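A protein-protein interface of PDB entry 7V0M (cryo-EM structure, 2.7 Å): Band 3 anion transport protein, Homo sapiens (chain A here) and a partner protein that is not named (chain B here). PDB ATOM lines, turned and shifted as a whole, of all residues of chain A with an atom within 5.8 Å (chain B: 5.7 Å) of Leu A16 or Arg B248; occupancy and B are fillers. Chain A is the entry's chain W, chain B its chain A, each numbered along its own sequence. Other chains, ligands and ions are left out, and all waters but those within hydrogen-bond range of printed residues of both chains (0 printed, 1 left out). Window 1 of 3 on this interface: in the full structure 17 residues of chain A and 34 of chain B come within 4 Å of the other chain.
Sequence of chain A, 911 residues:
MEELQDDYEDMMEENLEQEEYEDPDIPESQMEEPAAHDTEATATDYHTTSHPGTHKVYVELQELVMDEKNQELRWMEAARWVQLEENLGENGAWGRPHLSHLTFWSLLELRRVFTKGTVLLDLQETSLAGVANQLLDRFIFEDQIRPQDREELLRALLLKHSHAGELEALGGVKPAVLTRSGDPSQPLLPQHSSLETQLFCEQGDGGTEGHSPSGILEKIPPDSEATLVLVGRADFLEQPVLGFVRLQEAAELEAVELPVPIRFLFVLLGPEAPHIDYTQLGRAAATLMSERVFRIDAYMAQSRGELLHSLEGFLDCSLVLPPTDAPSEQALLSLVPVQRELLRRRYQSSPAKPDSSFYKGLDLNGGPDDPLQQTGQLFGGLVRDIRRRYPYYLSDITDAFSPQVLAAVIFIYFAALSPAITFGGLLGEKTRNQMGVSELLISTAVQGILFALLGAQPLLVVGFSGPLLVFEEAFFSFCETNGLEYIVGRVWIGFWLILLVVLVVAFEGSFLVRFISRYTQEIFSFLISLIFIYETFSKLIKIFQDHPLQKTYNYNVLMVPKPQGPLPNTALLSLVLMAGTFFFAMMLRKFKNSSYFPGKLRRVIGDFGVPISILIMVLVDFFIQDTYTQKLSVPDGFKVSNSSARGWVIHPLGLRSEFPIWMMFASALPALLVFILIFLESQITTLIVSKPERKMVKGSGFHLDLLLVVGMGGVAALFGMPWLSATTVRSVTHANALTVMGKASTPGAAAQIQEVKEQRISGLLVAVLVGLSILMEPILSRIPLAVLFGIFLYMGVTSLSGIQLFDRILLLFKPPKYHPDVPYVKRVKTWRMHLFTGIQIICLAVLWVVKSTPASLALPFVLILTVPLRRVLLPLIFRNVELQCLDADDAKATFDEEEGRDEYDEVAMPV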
ATOM      1  N   MET A  11       3.622  -6.304 -26.057  1.00  0.00           N
ATOM      2  CA  MET A  11       4.145  -6.536 -24.716  1.00  0.00           C
ATOM      3  C   MET A  11       4.432  -8.013 -24.486  1.00  0.00           C
ATOM      4  O   MET A  11       5.440  -8.365 -23.869  1.00  0.00           O
ATOM      5  CB  MET A  11       3.163  -6.013 -23.671  1.00  0.00           C
ATOM      6  CG  MET A  11       3.744  -5.525 -22.329  1.00  0.00           C
ATOM      7  SD  MET A  11       5.156  -4.380 -22.306  1.00  0.00           S
ATOM      8  CE  MET A  11       6.587  -5.440 -22.525  1.00  0.00           C
ATOM      9  N   MET A  12       3.552  -8.893 -24.971  1.00  0.00           N
ATOM     10  CA  MET A  12       3.788 -10.326 -24.831  1.00  0.00           C
ATOM     11  C   MET A  12       4.998 -10.774 -25.641  1.00  0.00           C
ATOM     12  O   MET A  12       5.769 -11.626 -25.190  1.00  0.00           O
ATOM     13  CB  MET A  12       2.545 -11.110 -25.245  1.00  0.00           C
ATOM     14  CG  MET A  12       2.444 -12.478 -24.591  1.00  0.00           C
ATOM     15  SD  MET A  12       3.071 -12.479 -22.903  1.00  0.00           S
ATOM     16  CE  MET A  12       1.558 -12.236 -21.986  1.00  0.00           C
ATOM     17  N   GLU A  13       5.174 -10.217 -26.840  1.00  0.00           N
ATOM     18  CA  GLU A  13       6.348 -10.539 -27.645  1.00  0.00           C
ATOM     19  C   GLU A  13       7.628 -10.112 -26.939  1.00  0.00           C
ATOM     20  O   GLU A  13       8.631 -10.834 -26.957  1.00  0.00           O
ATOM     21  CB  GLU A  13       6.241  -9.873 -29.015  1.00  0.00           C
ATOM     22  CG  GLU A  13       6.780 -10.714 -30.156  1.00  0.00           C
ATOM     23  CD  GLU A  13       7.374  -9.872 -31.266  1.00  0.00           C
ATOM     24  OE1 GLU A  13       6.732  -8.882 -31.672  1.00  0.00           O
ATOM     25  OE2 GLU A  13       8.486 -10.200 -31.731  1.00  0.00           O
ATOM     26  N   GLU A  14       7.613  -8.932 -26.315  1.00  0.00           N
ATOM     27  CA  GLU A  14       8.778  -8.498 -25.547  1.00  0.00           C
ATOM     28  C   GLU A  14       8.999  -9.383 -24.325  1.00  0.00           C
ATOM     29  O   GLU A  14      10.142  -9.699 -23.979  1.00  0.00           O
ATOM     30  CB  GLU A  14       8.622  -7.037 -25.131  1.00  0.00           C
ATOM     31  CG  GLU A  14       8.848  -6.044 -26.257  1.00  0.00           C
ATOM     32  CD  GLU A  14       9.400  -4.719 -25.766  1.00  0.00           C
ATOM     33  OE1 GLU A  14       8.875  -4.186 -24.766  1.00  0.00           O
ATOM     34  OE2 GLU A  14      10.361  -4.210 -26.382  1.00  0.00           O
ATOM     35  N   ASN A  15       7.916  -9.792 -23.661  1.00  0.00           N
ATOM     36  CA  ASN A  15       8.036 -10.592 -22.445  1.00  0.00           C
ATOM     37  C   ASN A  15       8.583 -11.983 -22.740  1.00  0.00           C
ATOM     38  O   ASN A  15       9.376 -12.520 -21.958  1.00  0.00           O
ATOM     39  CB  ASN A  15       6.679 -10.695 -21.748  1.00  0.00           C
ATOM     40  CG  ASN A  15       6.295  -9.420 -21.024  1.00  0.00           C
ATOM     41  OD1 ASN A  15       7.141  -8.744 -20.441  1.00  0.00           O
ATOM     42  ND2 ASN A  15       5.010  -9.094 -21.046  1.00  0.00           N
ATOM     43  N   LEU A  16       8.166 -12.586 -23.855  1.00  0.00           N
ATOM     44  CA  LEU A  16       8.576 -13.953 -24.156  1.00  0.00           C
ATOM     45  C   LEU A  16      10.049 -14.061 -24.527  1.00  0.00           C
ATOM     46  O   LEU A  16      10.611 -15.157 -24.437  1.00  0.00           O
ATOM     47  CB  LEU A  16       7.704 -14.526 -25.272  1.00  0.00           C
ATOM     48  CG  LEU A  16       6.247 -14.791 -24.886  1.00  0.00           C
ATOM     49  CD1 LEU A  16       5.406 -15.107 -26.112  1.00  0.00           C
ATOM     50  CD2 LEU A  16       6.149 -15.912 -23.866  1.00  0.00           C
ATOM     51  N   GLU A  17      10.679 -12.957 -24.941  1.00  0.00           N
ATOM     52  CA  GLU A  17      12.120 -12.882 -25.198  1.00  0.00           C
ATOM     53  C   GLU A  17      12.553 -13.923 -26.236  1.00  0.00           C
ATOM     54  O   GLU A  17      13.290 -14.869 -25.951  1.00  0.00           O
ATOM     55  CB  GLU A  17      12.918 -13.032 -23.898  1.00  0.00           C
ATOM     56  CG  GLU A  17      12.535 -12.046 -22.816  1.00  0.00           C
ATOM     57  CD  GLU A  17      13.421 -12.152 -21.593  1.00  0.00           C
ATOM     58  OE1 GLU A  17      13.052 -12.885 -20.652  1.00  0.00           O
ATOM     59  OE2 GLU A  17      14.488 -11.503 -21.573  1.00  0.00           O
ATOM     60  N   GLN A  18      12.061 -13.718 -27.461  1.00  0.00           N
ATOM     61  CA  GLN A  18      12.367 -14.638 -28.552  1.00  0.00           C
ATOM     62  C   GLN A  18      13.856 -14.668 -28.876  1.00  0.00           C
ATOM     63  O   GLN A  18      14.341 -15.641 -29.463  1.00  0.00           O
ATOM     64  CB  GLN A  18      11.562 -14.257 -29.793  1.00  0.00           C
ATOM     65  CG  GLN A  18      10.349 -15.133 -30.037  1.00  0.00           C
ATOM     66  CD  GLN A  18       9.286 -14.429 -30.851  1.00  0.00           C
ATOM     67  OE1 GLN A  18       8.574 -13.563 -30.344  1.00  0.00           O
ATOM     68  NE2 GLN A  18       9.174 -14.793 -32.122  1.00  0.00           N
ATOM     69  N   GLU A  20      16.189 -14.912 -26.718  1.00  0.00           N
ATOM     70  CA  GLU A  20      16.840 -15.797 -25.762  1.00  0.00           C
ATOM     71  C   GLU A  20      16.774 -17.263 -26.168  1.00  0.00           C
ATOM     72  O   GLU A  20      17.355 -18.106 -25.476  1.00  0.00           O
ATOM     73  CB  GLU A  20      16.225 -15.614 -24.373  1.00  0.00           C
ATOM     74  CG  GLU A  20      16.853 -14.488 -23.567  1.00  0.00           C
ATOM     75  CD  GLU A  20      18.369 -14.483 -23.656  1.00  0.00           C
ATOM     76  OE1 GLU A  20      19.000 -15.433 -23.143  1.00  0.00           O
ATOM     77  OE2 GLU A  20      18.929 -13.532 -24.240  1.00  0.00           O
ATOM     78  N   TYR A  21      16.078 -17.589 -27.258  1.00  0.00           N
ATOM     79  CA  TYR A  21      16.031 -18.944 -27.791  1.00  0.00           C
ATOM     80  C   TYR A  21      16.834 -19.074 -29.079  1.00  0.00           C
ATOM     81  O   TYR A  21      16.571 -19.972 -29.885  1.00  0.00           O
ATOM     82  CB  TYR A  21      14.583 -19.382 -28.019  1.00  0.00           C
ATOM     83  CG  TYR A  21      13.725 -19.307 -26.779  1.00  0.00           C
ATOM     84  CD1 TYR A  21      13.093 -18.123 -26.419  1.00  0.00           C
ATOM     85  CD2 TYR A  21      13.553 -20.415 -25.961  1.00  0.00           C
ATOM     86  CE1 TYR A  21      12.316 -18.047 -25.290  1.00  0.00           C
ATOM     87  CE2 TYR A  21      12.774 -20.347 -24.826  1.00  0.00           C
ATOM     88  CZ  TYR A  21      12.159 -19.161 -24.495  1.00  0.00           C
ATOM     89  OH  TYR A  21      11.382 -19.076 -23.367  1.00  0.00           O
ATOM     90  N   PHE B 207       2.186 -18.063 -30.955  1.00  0.00           N
ATOM     91  CA  PHE B 207       2.283 -18.808 -29.708  1.00  0.00           C
ATOM     92  C   PHE B 207       0.899 -19.185 -29.197  1.00  0.00           C
ATOM     93  O   PHE B 207      -0.006 -18.350 -29.140  1.00  0.00           O
ATOM     94  CB  PHE B 207       3.025 -17.989 -28.652  1.00  0.00           C
ATOM     95  CG  PHE B 207       4.508 -17.927 -28.863  1.00  0.00           C
ATOM     96  CD1 PHE B 207       5.301 -19.042 -28.650  1.00  0.00           C
ATOM     97  CD2 PHE B 207       5.113 -16.753 -29.280  1.00  0.00           C
ATOM     98  CE1 PHE B 207       6.665 -18.990 -28.843  1.00  0.00           C
ATOM     99  CE2 PHE B 207       6.478 -16.693 -29.476  1.00  0.00           C
ATOM    100  CZ  PHE B 207       7.256 -17.813 -29.258  1.00  0.00           C
ATOM    101  N   HIS B 211       2.007 -22.040 -24.483  1.00  0.00           N
ATOM    102  CA  HIS B 211       3.282 -21.332 -24.397  1.00  0.00           C
ATOM    103  C   HIS B 211       3.254 -20.284 -23.292  1.00  0.00           C
ATOM    104  O   HIS B 211       4.204 -20.160 -22.509  1.00  0.00           O
ATOM    105  CB  HIS B 211       3.605 -20.674 -25.740  1.00  0.00           C
ATOM    106  CG  HIS B 211       4.028 -21.633 -26.808  1.00  0.00           C
ATOM    107  ND1 HIS B 211       3.170 -22.074 -27.791  1.00  0.00           N
ATOM    108  CD2 HIS B 211       5.225 -22.210 -27.067  1.00  0.00           C
ATOM    109  CE1 HIS B 211       3.814 -22.898 -28.598  1.00  0.00           C
ATOM    110  NE2 HIS B 211       5.064 -22.994 -28.183  1.00  0.00           N
ATOM    111  N   ILE B 212       2.162 -19.517 -23.217  1.00  0.00           N
ATOM    112  CA  ILE B 212       2.028 -18.489 -22.188  1.00  0.00           C
ATOM    113  C   ILE B 212       1.974 -19.125 -20.806  1.00  0.00           C
ATOM    114  O   ILE B 212       2.582 -18.622 -19.853  1.00  0.00           O
ATOM    115  CB  ILE B 212       0.785 -17.621 -22.463  1.00  0.00           C
ATOM    116  CG1 ILE B 212       0.845 -17.023 -23.868  1.00  0.00           C
ATOM    117  CG2 ILE B 212       0.658 -16.522 -21.426  1.00  0.00           C
ATOM    118  CD1 ILE B 212       2.094 -16.230 -24.146  1.00  0.00           C
ATOM    119  N   HIS B 215       5.377 -20.121 -19.821  1.00  0.00           N
ATOM    120  CA  HIS B 215       6.237 -18.981 -19.510  1.00  0.00           C
ATOM    121  C   HIS B 215       6.074 -18.533 -18.064  1.00  0.00           C
ATOM    122  O   HIS B 215       7.066 -18.269 -17.373  1.00  0.00           O
ATOM    123  CB  HIS B 215       5.940 -17.829 -20.466  1.00  0.00           C
ATOM    124  CG  HIS B 215       6.767 -16.607 -20.216  1.00  0.00           C
ATOM    125  ND1 HIS B 215       7.951 -16.363 -20.878  1.00  0.00           N
ATOM    126  CD2 HIS B 215       6.582 -15.560 -19.380  1.00  0.00           C
ATOM    127  CE1 HIS B 215       8.460 -15.220 -20.459  1.00  0.00           C
ATOM    128  NE2 HIS B 215       7.648 -14.711 -19.549  1.00  0.00           N
ATOM    129  N   LEU B 243       8.046 -26.752 -23.976  1.00  0.00           N
ATOM    130  CA  LEU B 243       9.132 -27.298 -23.168  1.00  0.00           C
ATOM    131  C   LEU B 243      10.362 -26.399 -23.220  1.00  0.00           C
ATOM    132  O   LEU B 243      11.060 -26.236 -22.213  1.00  0.00           O
ATOM    133  CB  LEU B 243       9.477 -28.712 -23.629  1.00  0.00           C
ATOM    134  CG  LEU B 243      10.512 -29.469 -22.794  1.00  0.00           C
ATOM    135  CD1 LEU B 243      10.051 -29.602 -21.353  1.00  0.00           C
ATOM    136  CD2 LEU B 243      10.798 -30.834 -23.393  1.00  0.00           C
ATOM    137  N   HIS B 244      10.636 -25.801 -24.383  1.00  0.00           N
ATOM    138  CA  HIS B 244      11.736 -24.848 -24.497  1.00  0.00           C
ATOM    139  C   HIS B 244      11.536 -23.668 -23.557  1.00  0.00           C
ATOM    140  O   HIS B 244      12.463 -23.255 -22.854  1.00  0.00           O
ATOM    141  CB  HIS B 244      11.854 -24.347 -25.936  1.00  0.00           C
ATOM    142  CG  HIS B 244      12.574 -25.283 -26.852  1.00  0.00           C
ATOM    143  ND1 HIS B 244      11.914 -26.125 -27.718  1.00  0.00           N
ATOM    144  CD2 HIS B 244      13.895 -25.499 -27.048  1.00  0.00           C
ATOM    145  CE1 HIS B 244      12.797 -26.826 -28.404  1.00  0.00           C
ATOM    146  NE2 HIS B 244      14.006 -26.465 -28.018  1.00  0.00           N
ATOM    147  N   ILE B 245      10.324 -23.112 -23.539  1.00  0.00           N
ATOM    148  CA  ILE B 245      10.041 -21.954 -22.698  1.00  0.00           C
ATOM    149  C   ILE B 245      10.144 -22.329 -21.227  1.00  0.00           C
ATOM    150  O   ILE B 245      10.716 -21.590 -20.417  1.00  0.00           O
ATOM    151  CB  ILE B 245       8.657 -21.373 -23.038  1.00  0.00           C
ATOM    152  CG1 ILE B 245       8.649 -20.808 -24.453  1.00  0.00           C
ATOM    153  CG2 ILE B 245       8.305 -20.272 -22.083  1.00  0.00           C
ATOM    154  CD1 ILE B 245       7.281 -20.396 -24.932  1.00  0.00           C
ATOM    155  N   ALA B 246       9.600 -23.493 -20.863  1.00  0.00           N
ATOM    156  CA  ALA B 246       9.660 -23.935 -19.475  1.00  0.00           C
ATOM    157  C   ALA B 246      11.100 -24.166 -19.023  1.00  0.00           C
ATOM    158  O   ALA B 246      11.457 -23.843 -17.884  1.00  0.00           O
ATOM    159  CB  ALA B 246       8.822 -25.199 -19.296  1.00  0.00           C
ATOM    160  N   SER B 247      11.941 -24.724 -19.898  1.00  0.00           N
ATOM    161  CA  SER B 247      13.337 -24.949 -19.535  1.00  0.00           C
ATOM    162  C   SER B 247      14.111 -23.638 -19.449  1.00  0.00           C
ATOM    163  O   SER B 247      14.959 -23.471 -18.566  1.00  0.00           O
ATOM    164  CB  SER B 247      13.996 -25.894 -20.538  1.00  0.00           C
ATOM    165  OG  SER B 247      13.084 -26.881 -20.979  1.00  0.00           O
ATOM    166  N   ARG B 248      13.840 -22.702 -20.360  1.00  0.00           N
ATOM    167  CA  ARG B 248      14.521 -21.412 -20.330  1.00  0.00           C
ATOM    168  C   ARG B 248      14.135 -20.604 -19.097  1.00  0.00           C
ATOM    169  O   ARG B 248      14.981 -19.925 -18.504  1.00  0.00           O
ATOM    170  CB  ARG B 248      14.204 -20.629 -21.603  1.00  0.00           C
ATOM    171  CG  ARG B 248      15.290 -19.672 -22.055  1.00  0.00           C
ATOM    172  CD  ARG B 248      15.079 -18.285 -21.475  1.00  0.00           C
ATOM    173  NE  ARG B 248      13.779 -17.735 -21.834  1.00  0.00           N
ATOM    174  CZ  ARG B 248      13.393 -16.493 -21.576  1.00  0.00           C
ATOM    175  NH1 ARG B 248      14.181 -15.645 -20.938  1.00  0.00           N
ATOM    176  NH2 ARG B 248      12.186 -16.095 -21.963  1.00  0.00           N
ATOM    177  N   ARG B 249      12.865 -20.658 -18.700  1.00  0.00           N
ATOM    178  CA  ARG B 249      12.380 -19.851 -17.589  1.00  0.00           C
ATOM    179  C   ARG B 249      12.687 -20.457 -16.227  1.00  0.00           C
ATOM    180  O   ARG B 249      12.537 -19.764 -15.217  1.00  0.00           O
ATOM    181  CB  ARG B 249      10.870 -19.633 -17.723  1.00  0.00           C
ATOM    182  CG  ARG B 249      10.473 -18.737 -18.885  1.00  0.00           C
ATOM    183  CD  ARG B 249      10.560 -17.273 -18.511  1.00  0.00           C
ATOM    184  NE  ARG B 249       9.563 -16.915 -17.510  1.00  0.00           N
ATOM    185  CZ  ARG B 249       9.524 -15.755 -16.871  1.00  0.00           C
ATOM    186  NH1 ARG B 249      10.411 -14.805 -17.108  1.00  0.00           N
ATOM    187  NH2 ARG B 249       8.566 -15.541 -15.974  1.00  0.00           N
ATOM    188  N   GLY B 250      13.120 -21.711 -16.171  1.00  0.00           N
ATOM    189  CA  GLY B 250      13.383 -22.344 -14.895  1.00  0.00           C
ATOM    190  C   GLY B 250      12.162 -22.905 -14.207  1.00  0.00           C
ATOM    191  O   GLY B 250      12.171 -23.072 -12.984  1.00  0.00           O
ATOM    192  N   PRO B 275      15.877 -28.103 -25.585  1.00  0.00           N
ATOM    193  CA  PRO B 275      15.514 -27.615 -24.243  1.00  0.00           C
ATOM    194  C   PRO B 275      16.657 -27.689 -23.247  1.00  0.00           C
ATOM    195  O   PRO B 275      16.729 -26.856 -22.334  1.00  0.00           O
ATOM    196  CB  PRO B 275      14.351 -28.531 -23.844  1.00  0.00           C
ATOM    197  CG  PRO B 275      13.758 -28.953 -25.119  1.00  0.00           C
ATOM    198  CD  PRO B 275      14.891 -29.072 -26.094  1.00  0.00           C
ATOM    199  N   CYS B 278      18.538 -24.487 -23.566  1.00  0.00           N
ATOM    200  CA  CYS B 278      17.887 -23.387 -22.861  1.00  0.00           C
ATOM    201  C   CYS B 278      18.085 -23.497 -21.355  1.00  0.00           C
ATOM    202  O   CYS B 278      18.279 -22.486 -20.674  1.00  0.00           O
ATOM    203  CB  CYS B 278      16.401 -23.351 -23.211  1.00  0.00           C
ATOM    204  SG  CYS B 278      16.056 -23.258 -24.978  1.00  0.00           S
ATOM    205  N   ALA B 279      18.028 -24.716 -20.816  1.00  0.00           N
ATOM    206  CA  ALA B 279      18.233 -24.898 -19.382  1.00  0.00           C
ATOM    207  C   ALA B 279      19.669 -24.582 -18.979  1.00  0.00           C
ATOM    208  O   ALA B 279      19.909 -23.908 -17.973  1.00  0.00           O
ATOM    209  CB  ALA B 279      17.858 -26.324 -18.976  1.00  0.00           C
ATOM    210  N   ARG B 281      21.920 -22.754 -20.618  1.00  0.00           N
ATOM    211  CA  ARG B 281      22.259 -21.359 -20.868  1.00  0.00           C
ATOM    212  C   ARG B 281      21.855 -20.465 -19.703  1.00  0.00           C
ATOM    213  O   ARG B 281      22.573 -19.514 -19.374  1.00  0.00           O
ATOM    214  CB  ARG B 281      21.589 -20.893 -22.159  1.00  0.00           C
ATOM    215  CG  ARG B 281      21.859 -19.452 -22.531  1.00  0.00           C
ATOM    216  CD  ARG B 281      20.752 -18.921 -23.414  1.00  0.00           C
ATOM    217  NE  ARG B 281      20.981 -19.233 -24.819  1.00  0.00           N
ATOM    218  CZ  ARG B 281      20.922 -18.345 -25.801  1.00  0.00           C
ATOM    219  NH1 ARG B 281      20.637 -17.076 -25.568  1.00  0.00           N
ATOM    220  NH2 ARG B 281      21.154 -18.742 -27.049  1.00  0.00           N
ATOM    221  N   ASN B 282      20.719 -20.748 -19.071  1.00  0.00           N
ATOM    222  CA  ASN B 282      20.250 -19.986 -17.923  1.00  0.00           C
ATOM    223  C   ASN B 282      20.626 -20.632 -16.596  1.00  0.00           C
ATOM    224  O   ASN B 282      20.225 -20.132 -15.541  1.00  0.00           O
ATOM    225  CB  ASN B 282      18.738 -19.791 -18.007  1.00  0.00           C
ATOM    226  CG  ASN B 282      18.327 -18.990 -19.222  1.00  0.00           C
ATOM    227  OD1 ASN B 282      18.028 -19.549 -20.274  1.00  0.00           O
ATOM    228  ND2 ASN B 282      18.322 -17.673 -19.085  1.00  0.00           N
ATOM    229  N   HIS B 284      19.916 -23.667 -15.038  1.00  0.00           N
ATOM    230  CA  HIS B 284      18.911 -24.353 -14.232  1.00  0.00           C
ATOM    231  C   HIS B 284      19.369 -25.795 -14.049  1.00  0.00           C
ATOM    232  O   HIS B 284      19.195 -26.633 -14.934  1.00  0.00           O
ATOM    233  CB  HIS B 284      17.542 -24.263 -14.893  1.00  0.00           C
ATOM    234  CG  HIS B 284      17.078 -22.859 -15.115  1.00  0.00           C
ATOM    235  ND1 HIS B 284      17.052 -21.917 -14.110  1.00  0.00           N
ATOM    236  CD2 HIS B 284      16.639 -22.231 -16.231  1.00  0.00           C
ATOM    237  CE1 HIS B 284      16.606 -20.773 -14.594  1.00  0.00           C
ATOM    238  NE2 HIS B 284      16.348 -20.936 -15.879  1.00  0.00           N
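The side-chain carboxylate (OE1) of Glu A20 is in salt-bridge range of the guanidinium group (NH1) of Arg B281, 3.4 Å away. NE of Arg B248 is in hydrogen-bond range of OH of Tyr A21 (3.1 Å). OE1 of Glu A17 lies within salt-bridge range of NH1 of Arg B248, 3.0 Å away. O of Leu A16 lies within hydrogen-bond range of NH2 of Arg B248, at 3.1 Å.
The backbone carbonyl oxygen (O) of Cys B278 sits close to the side-chain amide oxygen (OD1) of Asn B282. O of Arg B248 is in hydrogen-bond range of NE2 of His B284. O of Met A11 is in hydrogen-bond range of ND2 of Asn A15, at 2.9 Å. O of His B215 lies within hydrogen-bond range of NE of Arg B249 (2.8 Å).
Among the printed residues, merely in contact across the chains: Met A12 with Ile B212 (3.8 Å), Asn A15 with His B215 (3.2 Å), Leu A16 with Phe B207 (3.6 Å), Leu A16 with His B215 (3.5 Å), Gln A18 with Phe B207 (3.9 Å), Glu A20 with Arg B248 (3.9 Å), Tyr A21 with His B244 (3.5 Å), Tyr A21 with Ile B245 (3.2 Å) and Tyr A21 with Cys B278 (3.9 Å).
Of the printed residues of chain B, Leu A16 touches Phe B207, His B215 and Arg B248. Of the printed residues of chain B, Gln A18 touches Phe B207 (3.9 Å). Pro B275 touches none of the printed residues of chain A. Printed residues of chain A within 4 Å of Cys B278: Tyr A21 (3.9 Å). The nearest printed residue of chain B that does not touch Leu A16 is Ile B212 (4.01 Å). The nearest residue of chain A that does not touch Arg B248 is Asn A15 (4.5 Å). The nearest printed residue of chain B that does not touch Met A12 is His B215 (5.9 Å).
Printed residues of chain B that touch a printed residue of chain A: Phe B207, Ile B212, His B215, His B244, Ile B245, Arg B248, Cys B278 and Arg B281. Hydrophobic or aromatic side chains of chain B within 4 Å of the printed part of chain A: Phe B207, Ile B212, His B215 and Ile B245. Of the 10 printed residues of chain A, 7 touch a printed residue of chain B. Hydrophobic or aromatic side chains of chain A that line the printed part of chain B: Met A12, Leu A16 and Tyr A21.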
